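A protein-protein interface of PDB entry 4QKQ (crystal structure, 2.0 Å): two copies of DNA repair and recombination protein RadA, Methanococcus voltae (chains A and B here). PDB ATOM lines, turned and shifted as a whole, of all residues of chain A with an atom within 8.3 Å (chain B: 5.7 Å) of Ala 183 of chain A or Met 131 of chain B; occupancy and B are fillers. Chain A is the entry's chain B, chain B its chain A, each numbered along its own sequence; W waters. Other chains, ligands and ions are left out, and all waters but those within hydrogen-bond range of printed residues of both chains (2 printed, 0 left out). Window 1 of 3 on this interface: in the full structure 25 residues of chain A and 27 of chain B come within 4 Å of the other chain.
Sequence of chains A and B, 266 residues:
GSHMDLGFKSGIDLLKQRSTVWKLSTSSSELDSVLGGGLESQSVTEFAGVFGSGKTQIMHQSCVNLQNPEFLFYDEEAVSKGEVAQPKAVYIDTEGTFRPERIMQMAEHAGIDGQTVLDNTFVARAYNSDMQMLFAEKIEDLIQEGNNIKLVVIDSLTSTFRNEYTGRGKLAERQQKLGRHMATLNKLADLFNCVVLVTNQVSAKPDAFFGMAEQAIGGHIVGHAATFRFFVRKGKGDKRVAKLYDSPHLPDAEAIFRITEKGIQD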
ATOM      1  N   LEU A   6      -5.854 -19.032  10.160  1.00  0.00           N
ATOM      2  CA  LEU A   6      -6.125 -19.549  11.495  1.00  0.00           C
ATOM      3  C   LEU A   6      -7.597 -19.880  11.759  1.00  0.00           C
ATOM      4  O   LEU A   6      -7.937 -20.368  12.836  1.00  0.00           O
ATOM      5  CB  LEU A   6      -5.606 -18.565  12.550  1.00  0.00           C
ATOM      6  CG  LEU A   6      -4.079 -18.438  12.680  1.00  0.00           C
ATOM      7  CD1 LEU A   6      -3.740 -17.131  13.381  1.00  0.00           C
ATOM      8  CD2 LEU A   6      -3.506 -19.626  13.442  1.00  0.00           C
ATOM      9  N   GLY A   7      -8.470 -19.618  10.788  1.00  0.00           N
ATOM     10  CA  GLY A   7      -9.883 -19.937  10.958  1.00  0.00           C
ATOM     11  C   GLY A   7     -10.751 -18.802  11.477  1.00  0.00           C
ATOM     12  O   GLY A   7     -11.963 -18.977  11.676  1.00  0.00           O
ATOM     13  N   PHE A   8     -10.129 -17.645  11.698  1.00  0.00           N
ATOM     14  CA  PHE A   8     -10.821 -16.452  12.188  1.00  0.00           C
ATOM     15  C   PHE A   8     -11.245 -15.583  11.000  1.00  0.00           C
ATOM     16  O   PHE A   8     -10.546 -15.526  10.000  1.00  0.00           O
ATOM     17  CB  PHE A   8      -9.882 -15.612  13.079  1.00  0.00           C
ATOM     18  CG  PHE A   8      -9.388 -16.330  14.309  1.00  0.00           C
ATOM     19  CD1 PHE A   8     -10.208 -16.481  15.424  1.00  0.00           C
ATOM     20  CD2 PHE A   8      -8.102 -16.864  14.347  1.00  0.00           C
ATOM     21  CE1 PHE A   8      -9.754 -17.155  16.561  1.00  0.00           C
ATOM     22  CE2 PHE A   8      -7.645 -17.531  15.471  1.00  0.00           C
ATOM     23  CZ  PHE A   8      -8.475 -17.677  16.582  1.00  0.00           C
ATOM     24  N   VAL A  44     -25.267 -25.466   5.772  1.00  0.00           N
ATOM     25  CA  VAL A  44     -25.670 -26.862   5.748  1.00  0.00           C
ATOM     26  C   VAL A  44     -27.175 -26.839   5.977  1.00  0.00           C
ATOM     27  O   VAL A  44     -27.670 -26.193   6.908  1.00  0.00           O
ATOM     28  CB  VAL A  44     -24.993 -27.701   6.862  1.00  0.00           C
ATOM     29  CG1 VAL A  44     -25.627 -29.085   6.919  1.00  0.00           C
ATOM     30  CG2 VAL A  44     -23.516 -27.841   6.580  1.00  0.00           C
ATOM     31  N   MET A 133     -16.922 -39.938   6.242  1.00  0.00           N
ATOM     32  CA  MET A 133     -16.165 -38.770   6.651  1.00  0.00           C
ATOM     33  C   MET A 133     -14.992 -38.536   5.740  1.00  0.00           C
ATOM     34  O   MET A 133     -14.680 -37.392   5.423  1.00  0.00           O
ATOM     35  CB  MET A 133     -15.693 -38.929   8.116  1.00  0.00           C
ATOM     36  CG  MET A 133     -16.853 -38.895   9.103  1.00  0.00           C
ATOM     37  SD  MET A 133     -16.436 -39.168  10.851  1.00  0.00           S
ATOM     38  CE  MET A 133     -15.462 -37.602  11.161  1.00  0.00           C
ATOM     39  N   ALA A 136     -16.051 -36.923   2.448  1.00  0.00           N
ATOM     40  CA  ALA A 136     -16.360 -35.517   2.683  1.00  0.00           C
ATOM     41  C   ALA A 136     -15.084 -34.695   2.593  1.00  0.00           C
ATOM     42  O   ALA A 136     -15.020 -33.699   1.872  1.00  0.00           O
ATOM     43  CB  ALA A 136     -17.013 -35.343   4.052  1.00  0.00           C
ATOM     44  N   GLU A 137     -14.056 -35.131   3.310  1.00  0.00           N
ATOM     45  CA  GLU A 137     -12.781 -34.425   3.290  1.00  0.00           C
ATOM     46  C   GLU A 137     -12.112 -34.444   1.919  1.00  0.00           C
ATOM     47  O   GLU A 137     -11.476 -33.472   1.526  1.00  0.00           O
ATOM     48  CB  GLU A 137     -11.842 -35.027   4.331  1.00  0.00           C
ATOM     49  CG  GLU A 137     -12.271 -34.757   5.754  1.00  0.00           C
ATOM     50  CD  GLU A 137     -11.425 -35.519   6.761  1.00  0.00           C
ATOM     51  OE1 GLU A 137     -11.776 -35.540   7.967  1.00  0.00           O
ATOM     52  OE2 GLU A 137     -10.401 -36.099   6.339  1.00  0.00           O
ATOM     53  N   GLN A 176     -18.964 -37.201  19.231  1.00  0.00           N
ATOM     54  CA  GLN A 176     -17.740 -36.520  18.854  1.00  0.00           C
ATOM     55  C   GLN A 176     -17.356 -36.783  17.397  1.00  0.00           C
ATOM     56  O   GLN A 176     -16.837 -35.900  16.720  1.00  0.00           O
ATOM     57  CB  GLN A 176     -16.599 -36.958  19.764  1.00  0.00           C
ATOM     58  CG  GLN A 176     -16.784 -36.539  21.222  1.00  0.00           C
ATOM     59  CD  GLN A 176     -15.774 -37.217  22.134  1.00  0.00           C
ATOM     60  OE1 GLN A 176     -14.569 -37.201  21.867  1.00  0.00           O
ATOM     61  NE2 GLN A 176     -16.262 -37.822  23.213  1.00  0.00           N
ATOM     62  N   LYS A 177     -17.589 -37.997  16.912  1.00  0.00           N
ATOM     63  CA  LYS A 177     -17.242 -38.277  15.516  1.00  0.00           C
ATOM     64  C   LYS A 177     -18.177 -37.409  14.668  1.00  0.00           C
ATOM     65  O   LYS A 177     -17.764 -36.780  13.711  1.00  0.00           O
ATOM     66  CB  LYS A 177     -17.444 -39.769  15.209  1.00  0.00           C
ATOM     67  CG  LYS A 177     -16.464 -40.335  14.208  1.00  0.00           C
ATOM     68  CD  LYS A 177     -16.732 -41.833  13.952  1.00  0.00           C
ATOM     69  CE  LYS A 177     -15.801 -42.404  12.891  1.00  0.00           C
ATOM     70  NZ  LYS A 177     -15.930 -43.885  12.754  1.00  0.00           N
ATOM     71  N   LEU A 178     -19.441 -37.379  15.064  1.00  0.00           N
ATOM     72  CA  LEU A 178     -20.472 -36.599  14.396  1.00  0.00           C
ATOM     73  C   LEU A 178     -20.069 -35.126  14.344  1.00  0.00           C
ATOM     74  O   LEU A 178     -20.183 -34.462  13.301  1.00  0.00           O
ATOM     75  CB  LEU A 178     -21.762 -36.746  15.182  1.00  0.00           C
ATOM     76  CG  LEU A 178     -23.047 -37.092  14.457  1.00  0.00           C
ATOM     77  CD1 LEU A 178     -22.766 -38.167  13.453  1.00  0.00           C
ATOM     78  CD2 LEU A 178     -24.096 -37.542  15.468  1.00  0.00           C
ATOM     79  N   GLY A 179     -19.595 -34.618  15.483  1.00  0.00           N
ATOM     80  CA  GLY A 179     -19.182 -33.231  15.558  1.00  0.00           C
ATOM     81  C   GLY A 179     -18.086 -32.895  14.590  1.00  0.00           C
ATOM     82  O   GLY A 179     -18.096 -31.828  13.969  1.00  0.00           O
ATOM     83  N   ARG A 180     -17.125 -33.805  14.449  1.00  0.00           N
ATOM     84  CA  ARG A 180     -16.010 -33.608  13.517  1.00  0.00           C
ATOM     85  C   ARG A 180     -16.551 -33.544  12.082  1.00  0.00           C
ATOM     86  O   ARG A 180     -16.165 -32.688  11.298  1.00  0.00           O
ATOM     87  CB  ARG A 180     -15.033 -34.775  13.639  1.00  0.00           C
ATOM     88  CG  ARG A 180     -13.777 -34.720  12.785  1.00  0.00           C
ATOM     89  CD  ARG A 180     -12.535 -35.108  13.635  1.00  0.00           C
ATOM     90  NE  ARG A 180     -12.895 -35.979  14.756  1.00  0.00           N
ATOM     91  CZ  ARG A 180     -13.116 -37.290  14.652  1.00  0.00           C
ATOM     92  NH1 ARG A 180     -13.454 -37.996  15.731  1.00  0.00           N
ATOM     93  NH2 ARG A 180     -12.973 -37.905  13.475  1.00  0.00           N
ATOM     94  N   HIS A 181     -17.439 -34.472  11.744  1.00  0.00           N
ATOM     95  CA  HIS A 181     -18.019 -34.507  10.402  1.00  0.00           C
ATOM     96  C   HIS A 181     -18.823 -33.212  10.137  1.00  0.00           C
ATOM     97  O   HIS A 181     -18.698 -32.613   9.074  1.00  0.00           O
ATOM     98  CB  HIS A 181     -18.900 -35.756  10.261  1.00  0.00           C
ATOM     99  CG  HIS A 181     -19.399 -35.987   8.866  1.00  0.00           C
ATOM    100  ND1 HIS A 181     -20.669 -36.446   8.595  1.00  0.00           N
ATOM    101  CD2 HIS A 181     -18.790 -35.837   7.669  1.00  0.00           C
ATOM    102  CE1 HIS A 181     -20.823 -36.569   7.289  1.00  0.00           C
ATOM    103  NE2 HIS A 181     -19.696 -36.208   6.706  1.00  0.00           N
ATOM    104  N   MET A 182     -19.630 -32.761  11.098  1.00  0.00           N
ATOM    105  CA  MET A 182     -20.388 -31.522  10.886  1.00  0.00           C
ATOM    106  C   MET A 182     -19.448 -30.361  10.619  1.00  0.00           C
ATOM    107  O   MET A 182     -19.734 -29.500   9.782  1.00  0.00           O
ATOM    108  CB  MET A 182     -21.288 -31.175  12.090  1.00  0.00           C
ATOM    109  CG  MET A 182     -22.427 -32.154  12.346  1.00  0.00           C
ATOM    110  SD  MET A 182     -23.516 -32.323  10.893  1.00  0.00           S
ATOM    111  CE  MET A 182     -24.221 -30.674  10.774  1.00  0.00           C
ATOM    112  N   ALA A 183     -18.316 -30.328  11.318  1.00  0.00           N
ATOM    113  CA  ALA A 183     -17.343 -29.249  11.112  1.00  0.00           C
ATOM    114  C   ALA A 183     -16.816 -29.269   9.672  1.00  0.00           C
ATOM    115  O   ALA A 183     -16.671 -28.239   9.032  1.00  0.00           O
ATOM    116  CB  ALA A 183     -16.161 -29.396  12.086  1.00  0.00           C
ATOM    117  N   THR A 184     -16.502 -30.455   9.184  1.00  0.00           N
ATOM    118  CA  THR A 184     -16.002 -30.582   7.835  1.00  0.00           C
ATOM    119  C   THR A 184     -17.052 -30.104   6.809  1.00  0.00           C
ATOM    120  O   THR A 184     -16.728 -29.353   5.884  1.00  0.00           O
ATOM    121  CB  THR A 184     -15.617 -32.047   7.556  1.00  0.00           C
ATOM    122  OG1 THR A 184     -14.533 -32.417   8.422  1.00  0.00           O
ATOM    123  CG2 THR A 184     -15.180 -32.228   6.116  1.00  0.00           C
ATOM    124  N   LEU A 185     -18.307 -30.514   6.993  1.00  0.00           N
ATOM    125  CA  LEU A 185     -19.353 -30.120   6.059  1.00  0.00           C
ATOM    126  C   LEU A 185     -19.481 -28.598   6.032  1.00  0.00           C
ATOM    127  O   LEU A 185     -19.602 -27.986   4.960  1.00  0.00           O
ATOM    128  CB  LEU A 185     -20.669 -30.766   6.453  1.00  0.00           C
ATOM    129  CG  LEU A 185     -20.617 -32.301   6.391  1.00  0.00           C
ATOM    130  CD1 LEU A 185     -21.941 -32.897   6.860  1.00  0.00           C
ATOM    131  CD2 LEU A 185     -20.306 -32.725   4.966  1.00  0.00           C
ATOM    132  N   ASN A 186     -19.427 -27.983   7.209  1.00  0.00           N
ATOM    133  CA  ASN A 186     -19.531 -26.533   7.304  1.00  0.00           C
ATOM    134  C   ASN A 186     -18.355 -25.849   6.663  1.00  0.00           C
ATOM    135  O   ASN A 186     -18.499 -24.803   6.023  1.00  0.00           O
ATOM    136  CB  ASN A 186     -19.658 -26.114   8.771  1.00  0.00           C
ATOM    137  CG  ASN A 186     -21.073 -26.044   9.200  1.00  0.00           C
ATOM    138  OD1 ASN A 186     -21.757 -25.069   8.909  1.00  0.00           O
ATOM    139  ND2 ASN A 186     -21.555 -27.085   9.861  1.00  0.00           N
ATOM    140  N   LYS A 187     -17.187 -26.454   6.827  1.00  0.00           N
ATOM    141  CA  LYS A 187     -15.964 -25.914   6.259  1.00  0.00           C
ATOM    142  C   LYS A 187     -16.028 -25.903   4.722  1.00  0.00           C
ATOM    143  O   LYS A 187     -15.679 -24.908   4.084  1.00  0.00           O
ATOM    144  CB  LYS A 187     -14.772 -26.743   6.730  1.00  0.00           C
ATOM    145  CG  LYS A 187     -13.441 -26.309   6.160  1.00  0.00           C
ATOM    146  CD  LYS A 187     -12.359 -27.328   6.488  1.00  0.00           C
ATOM    147  CE  LYS A 187     -11.059 -27.033   5.744  1.00  0.00           C
ATOM    148  NZ  LYS A 187     -10.047 -28.135   5.911  1.00  0.00           N
ATOM    149  N   LEU A 188     -16.467 -26.994   4.106  1.00  0.00           N
ATOM    150  CA  LEU A 188     -16.520 -26.937   2.653  1.00  0.00           C
ATOM    151  C   LEU A 188     -17.609 -25.989   2.151  1.00  0.00           C
ATOM    152  O   LEU A 188     -17.417 -25.295   1.146  1.00  0.00           O
ATOM    153  CB  LEU A 188     -16.634 -28.338   2.047  1.00  0.00           C
ATOM    154  CG  LEU A 188     -17.503 -29.385   2.675  1.00  0.00           C
ATOM    155  CD1 LEU A 188     -18.918 -29.169   2.184  1.00  0.00           C
ATOM    156  CD2 LEU A 188     -17.003 -30.762   2.291  1.00  0.00           C
ATOM    157  N   ALA A 189     -18.726 -25.913   2.865  1.00  0.00           N
ATOM    158  CA  ALA A 189     -19.794 -24.997   2.474  1.00  0.00           C
ATOM    159  C   ALA A 189     -19.232 -23.585   2.450  1.00  0.00           C
ATOM    160  O   ALA A 189     -19.417 -22.843   1.492  1.00  0.00           O
ATOM    161  CB  ALA A 189     -20.950 -25.059   3.469  1.00  0.00           C
ATOM    162  N   ASP A 190     -18.529 -23.237   3.519  1.00  0.00           N
ATOM    163  CA  ASP A 190     -17.946 -21.917   3.678  1.00  0.00           C
ATOM    164  C   ASP A 190     -16.774 -21.610   2.754  1.00  0.00           C
ATOM    165  O   ASP A 190     -16.819 -20.654   1.986  1.00  0.00           O
ATOM    166  CB  ASP A 190     -17.506 -21.731   5.137  1.00  0.00           C
ATOM    167  CG  ASP A 190     -16.703 -20.465   5.341  1.00  0.00           C
ATOM    168  OD1 ASP A 190     -15.468 -20.559   5.523  1.00  0.00           O
ATOM    169  OD2 ASP A 190     -17.311 -19.373   5.303  1.00  0.00           O
ATOM    170  N   LEU A 191     -15.725 -22.425   2.817  1.00  0.00           N
ATOM    171  CA  LEU A 191     -14.541 -22.176   1.998  1.00  0.00           C
ATOM    172  C   LEU A 191     -14.754 -22.272   0.490  1.00  0.00           C
ATOM    173  O   LEU A 191     -14.159 -21.513  -0.268  1.00  0.00           O
ATOM    174  CB  LEU A 191     -13.404 -23.116   2.409  1.00  0.00           C
ATOM    175  CG  LEU A 191     -13.050 -23.102   3.911  1.00  0.00           C
ATOM    176  CD1 LEU A 191     -11.849 -23.986   4.135  1.00  0.00           C
ATOM    177  CD2 LEU A 191     -12.748 -21.679   4.395  1.00  0.00           C
ATOM    178  N   ILE A 221     -25.504 -31.725  18.723  1.00  0.00           N
ATOM    179  CA  ILE A 221     -24.220 -31.721  18.047  1.00  0.00           C
ATOM    180  C   ILE A 221     -24.439 -31.448  16.552  1.00  0.00           C
ATOM    181  O   ILE A 221     -23.653 -30.744  15.905  1.00  0.00           O
ATOM    182  CB  ILE A 221     -23.479 -33.070  18.273  1.00  0.00           C
ATOM    183  CG1 ILE A 221     -22.167 -32.800  18.987  1.00  0.00           C
ATOM    184  CG2 ILE A 221     -23.203 -33.785  16.972  1.00  0.00           C
ATOM    185  CD1 ILE A 221     -21.319 -31.803  18.302  1.00  0.00           C
ATOM    186  N   ALA A 225     -24.994 -27.208  14.399  1.00  0.00           N
ATOM    187  CA  ALA A 225     -24.147 -27.050  13.216  1.00  0.00           C
ATOM    188  C   ALA A 225     -24.898 -27.016  11.864  1.00  0.00           C
ATOM    189  O   ALA A 225     -24.283 -26.871  10.818  1.00  0.00           O
ATOM    190  CB  ALA A 225     -23.094 -28.145  13.206  1.00  0.00           C
ATOM    191  N   ARG B 125     -16.171 -19.551  14.499  1.00  0.00           N
ATOM    192  CA  ARG B 125     -17.314 -20.426  14.659  1.00  0.00           C
ATOM    193  C   ARG B 125     -16.800 -21.824  15.020  1.00  0.00           C
ATOM    194  O   ARG B 125     -16.160 -22.476  14.212  1.00  0.00           O
ATOM    195  CB  ARG B 125     -18.126 -20.456  13.350  1.00  0.00           C
ATOM    196  CG  ARG B 125     -19.417 -21.266  13.416  1.00  0.00           C
ATOM    197  CD  ARG B 125     -20.446 -20.562  14.263  1.00  0.00           C
ATOM    198  NE  ARG B 125     -21.690 -21.327  14.364  1.00  0.00           N
ATOM    199  CZ  ARG B 125     -21.860 -22.381  15.157  1.00  0.00           C
ATOM    200  NH1 ARG B 125     -23.019 -23.008  15.184  1.00  0.00           N
ATOM    201  NH2 ARG B 125     -20.874 -22.799  15.938  1.00  0.00           N
ATOM    202  N   ALA B 126     -17.066 -22.273  16.245  1.00  0.00           N
ATOM    203  CA  ALA B 126     -16.622 -23.597  16.689  1.00  0.00           C
ATOM    204  C   ALA B 126     -17.809 -24.561  16.714  1.00  0.00           C
ATOM    205  O   ALA B 126     -18.811 -24.304  17.399  1.00  0.00           O
ATOM    206  CB  ALA B 126     -15.984 -23.503  18.095  1.00  0.00           C
ATOM    207  N   TYR B 127     -17.693 -25.663  15.971  1.00  0.00           N
ATOM    208  CA  TYR B 127     -18.763 -26.671  15.887  1.00  0.00           C
ATOM    209  C   TYR B 127     -18.623 -27.846  16.871  1.00  0.00           C
ATOM    210  O   TYR B 127     -19.548 -28.637  17.045  1.00  0.00           O
ATOM    211  CB  TYR B 127     -18.853 -27.214  14.447  1.00  0.00           C
ATOM    212  CG  TYR B 127     -19.210 -26.154  13.427  1.00  0.00           C
ATOM    213  CD1 TYR B 127     -20.513 -25.660  13.339  1.00  0.00           C
ATOM    214  CD2 TYR B 127     -18.248 -25.640  12.560  1.00  0.00           C
ATOM    215  CE1 TYR B 127     -20.853 -24.681  12.403  1.00  0.00           C
ATOM    216  CE2 TYR B 127     -18.571 -24.656  11.622  1.00  0.00           C
ATOM    217  CZ  TYR B 127     -19.881 -24.187  11.553  1.00  0.00           C
ATOM    218  OH  TYR B 127     -20.226 -23.244  10.620  1.00  0.00           O
ATOM    219  N   ASN B 128     -17.474 -27.969  17.516  1.00  0.00           N
ATOM    220  CA  ASN B 128     -17.274 -29.040  18.497  1.00  0.00           C
ATOM    221  C   ASN B 128     -16.229 -28.573  19.500  1.00  0.00           C
ATOM    222  O   ASN B 128     -15.569 -27.574  19.264  1.00  0.00           O
ATOM    223  CB  ASN B 128     -16.778 -30.332  17.838  1.00  0.00           C
ATOM    224  CG  ASN B 128     -15.603 -30.104  16.929  1.00  0.00           C
ATOM    225  OD1 ASN B 128     -15.744 -30.142  15.705  1.00  0.00           O
ATOM    226  ND2 ASN B 128     -14.436 -29.859  17.503  1.00  0.00           N
ATOM    227  N   SER B 129     -16.081 -29.305  20.600  1.00  0.00           N
ATOM    228  CA  SER B 129     -15.109 -28.926  21.649  1.00  0.00           C
ATOM    229  C   SER B 129     -13.673 -28.781  21.164  1.00  0.00           C
ATOM    230  O   SER B 129     -12.971 -27.853  21.579  1.00  0.00           O
ATOM    231  CB  SER B 129     -15.177 -29.921  22.813  1.00  0.00           C
ATOM    232  OG  SER B 129     -14.670 -31.182  22.426  1.00  0.00           O
ATOM    233  N   ASP B 130     -13.212 -29.688  20.302  1.00  0.00           N
ATOM    234  CA  ASP B 130     -11.858 -29.578  19.766  1.00  0.00           C
ATOM    235  C   ASP B 130     -11.611 -28.218  19.084  1.00  0.00           C
ATOM    236  O   ASP B 130     -10.595 -27.566  19.356  1.00  0.00           O
ATOM    237  CB  ASP B 130     -11.545 -30.674  18.728  1.00  0.00           C
ATOM    238  CG  ASP B 130     -11.341 -32.046  19.343  1.00  0.00           C
ATOM    239  OD1 ASP B 130     -10.951 -32.137  20.531  1.00  0.00           O
ATOM    240  OD2 ASP B 130     -11.555 -33.042  18.611  1.00  0.00           O
ATOM    241  N   MET B 131     -12.510 -27.799  18.182  1.00  0.00           N
ATOM    242  CA  MET B 131     -12.339 -26.513  17.488  1.00  0.00           C
ATOM    243  C   MET B 131     -12.350 -25.378  18.515  1.00  0.00           C
ATOM    244  O   MET B 131     -11.568 -24.450  18.435  1.00  0.00           O
ATOM    245  CB  MET B 131     -13.492 -26.223  16.486  1.00  0.00           C
ATOM    246  CG  MET B 131     -13.594 -27.134  15.287  1.00  0.00           C
ATOM    247  SD  MET B 131     -14.938 -26.577  14.163  1.00  0.00           S
ATOM    248  CE  MET B 131     -14.123 -25.256  13.317  1.00  0.00           C
ATOM    249  N   GLN B 132     -13.294 -25.451  19.439  1.00  0.00           N
ATOM    250  CA  GLN B 132     -13.419 -24.443  20.471  1.00  0.00           C
ATOM    251  C   GLN B 132     -12.104 -24.280  21.207  1.00  0.00           C
ATOM    252  O   GLN B 132     -11.615 -23.174  21.377  1.00  0.00           O
ATOM    253  CB  GLN B 132     -14.499 -24.835  21.467  1.00  0.00           C
ATOM    254  CG  GLN B 132     -14.631 -23.837  22.606  1.00  0.00           C
ATOM    255  CD  GLN B 132     -15.752 -24.186  23.537  1.00  0.00           C
ATOM    256  OE1 GLN B 132     -16.748 -24.780  23.132  1.00  0.00           O
ATOM    257  NE2 GLN B 132     -15.618 -23.797  24.789  1.00  0.00           N
ATOM    258  N   MET B 133     -11.531 -25.401  21.619  1.00  0.00           N
ATOM    259  CA  MET B 133     -10.289 -25.400  22.361  1.00  0.00           C
ATOM    260  C   MET B 133      -9.109 -24.974  21.527  1.00  0.00           C
ATOM    261  O   MET B 133      -8.235 -24.273  22.018  1.00  0.00           O
ATOM    262  CB  MET B 133     -10.063 -26.785  22.961  1.00  0.00           C
ATOM    263  CG  MET B 133     -11.106 -27.100  24.040  1.00  0.00           C
ATOM    264  SD  MET B 133     -10.767 -28.619  24.929  1.00  0.00           S
ATOM    265  CE  MET B 133      -9.083 -28.318  25.415  1.00  0.00           C
ATOM    266  N   LEU B 134      -9.079 -25.367  20.258  1.00  0.00           N
ATOM    267  CA  LEU B 134      -7.959 -24.984  19.411  1.00  0.00           C
ATOM    268  C   LEU B 134      -8.013 -23.489  19.075  1.00  0.00           C
ATOM    269  O   LEU B 134      -6.985 -22.824  18.999  1.00  0.00           O
ATOM    270  CB  LEU B 134      -7.945 -25.823  18.136  1.00  0.00           C
ATOM    271  CG  LEU B 134      -6.816 -25.570  17.139  1.00  0.00           C
ATOM    272  CD1 LEU B 134      -5.468 -25.822  17.804  1.00  0.00           C
ATOM    273  CD2 LEU B 134      -7.001 -26.487  15.922  1.00  0.00           C
ATOM    274  N   PHE B 135      -9.211 -22.961  18.874  1.00  0.00           N
ATOM    275  CA  PHE B 135      -9.350 -21.538  18.580  1.00  0.00           C
ATOM    276  C   PHE B 135      -8.741 -20.714  19.737  1.00  0.00           C
ATOM    277  O   PHE B 135      -8.012 -19.759  19.495  1.00  0.00           O
ATOM    278  CB  PHE B 135     -10.830 -21.186  18.382  1.00  0.00           C
ATOM    279  CG  PHE B 135     -11.327 -21.372  16.944  1.00  0.00           C
ATOM    280  CD1 PHE B 135     -12.607 -21.847  16.688  1.00  0.00           C
ATOM    281  CD2 PHE B 135     -10.529 -21.019  15.871  1.00  0.00           C
ATOM    282  CE1 PHE B 135     -13.086 -21.961  15.359  1.00  0.00           C
ATOM    283  CE2 PHE B 135     -10.995 -21.128  14.542  1.00  0.00           C
ATOM    284  CZ  PHE B 135     -12.273 -21.595  14.291  1.00  0.00           C
ATOM    285  N   ALA B 136      -9.037 -21.099  20.980  1.00  0.00           N
ATOM    286  CA  ALA B 136      -8.507 -20.388  22.146  1.00  0.00           C
ATOM    287  C   ALA B 136      -6.991 -20.425  22.121  1.00  0.00           C
ATOM    288  O   ALA B 136      -6.334 -19.417  22.345  1.00  0.00           O
ATOM    289  CB  ALA B 136      -9.033 -21.008  23.439  1.00  0.00           C
HETATM  290  O   HOH W   1     -21.449 -22.802   7.557  1.00  0.00           O
HETATM  291  O   HOH W   2     -22.376 -28.432  16.768  1.00  0.00           O
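The side-chain amide oxygen (OD1) of Asn 186 of chain A is in hydrogen-bond range of the side-chain hydroxyl (OH) of Tyr 127 of chain B, at 2.9 Å. OD1 of Asn 128 of chain B sits close to O of Gly 179 of chain A.
Positions printed for both chains: 133 and 136. Of the 10 pairs that touch across the chains among the printed residues, none has its exchanged pair printed and touching as well.
Printed residues of chain B that touch a printed residue of chain A: Tyr 127, Asn 128, Met 131 and Phe 135. Among the printed residues, 10 pairs touch across the chains. Among the printed residues, no Asp or Glu carboxylate lies within 4 Å of a Lys or Arg side-chain nitrogen of the other chain.
The backbone NH (N) of Met 131 of chain B sits close to the side-chain amide nitrogen (ND2) of Asn 128 of chain B. The backbone carbonyl oxygen of Met 182 of chain A lies within hydrogen-bond range of the side-chain amide nitrogen of Asn 186 of chain A (3.0 Å). ND2 of Asn 128 of chain B sits close to N of Asp 130 of chain B (3.1 Å). N of Tyr 127 of chain B sits at hydrogen-bond distance from SD of Met 131 of chain B. The backbone carbonyl oxygen (O) of Ala 225 of chain A sits at hydrogen-bond distance from the side-chain amide nitrogen (ND2) of Asn 186 of chain A (2.9 Å).
Of the printed residues of chain B, Ala 183 of chain A touches Tyr 127, Asn 128 and Met 131. Printed residues of chain B within 4 Å of Ile 221 of chain A: Tyr 127. Of the printed residues of chain B, Ala 225 of chain A touches Tyr 127. Of the printed residues of chain A, Phe 135 of chain B touches Leu 6 (3.6 Å), Gly 7 (3.7 Å) and Phe 8 (3.6 Å). Of the printed residues of chain B, Asn 186 of chain A touches Tyr 127. Of the printed residues of chain B, Gly 179 of chain A touches Asn 128 (3.4 Å). The nearest printed residue of chain B that does not touch Leu 6 of chain A is Leu 134 of chain B (6.7 Å).
Among the printed residues, merely in contact across the chains: Leu 6 of chain A with Phe 135 of chain B (3.6 Å), Gly 7 of chain A with Phe 135 of chain B (3.7 Å), Phe 8 of chain A with Phe 135 of chain B (3.6 Å), Ala 183 of chain A with Tyr 127 of chain B (3.99 Å), Ala 183 of chain A with Asn 128 of chain B (3.7 Å), Ala 183 of chain A with Met 131 of chain B (3.7 Å), Ile 221 of chain A with Tyr 127 of chain B (3.8 Å) and Ala 225 of chain A with Tyr 127 of chain B (3.6 Å).
Water W1 bridges OD1 of Asn 186 of chain A and OH of Tyr 127 of chain B. Water W2 lies within hydrogen-bond range of O of Ile 221 of chain A (2.8 Å) and O of Tyr 127 of chain B (2.8 Å).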
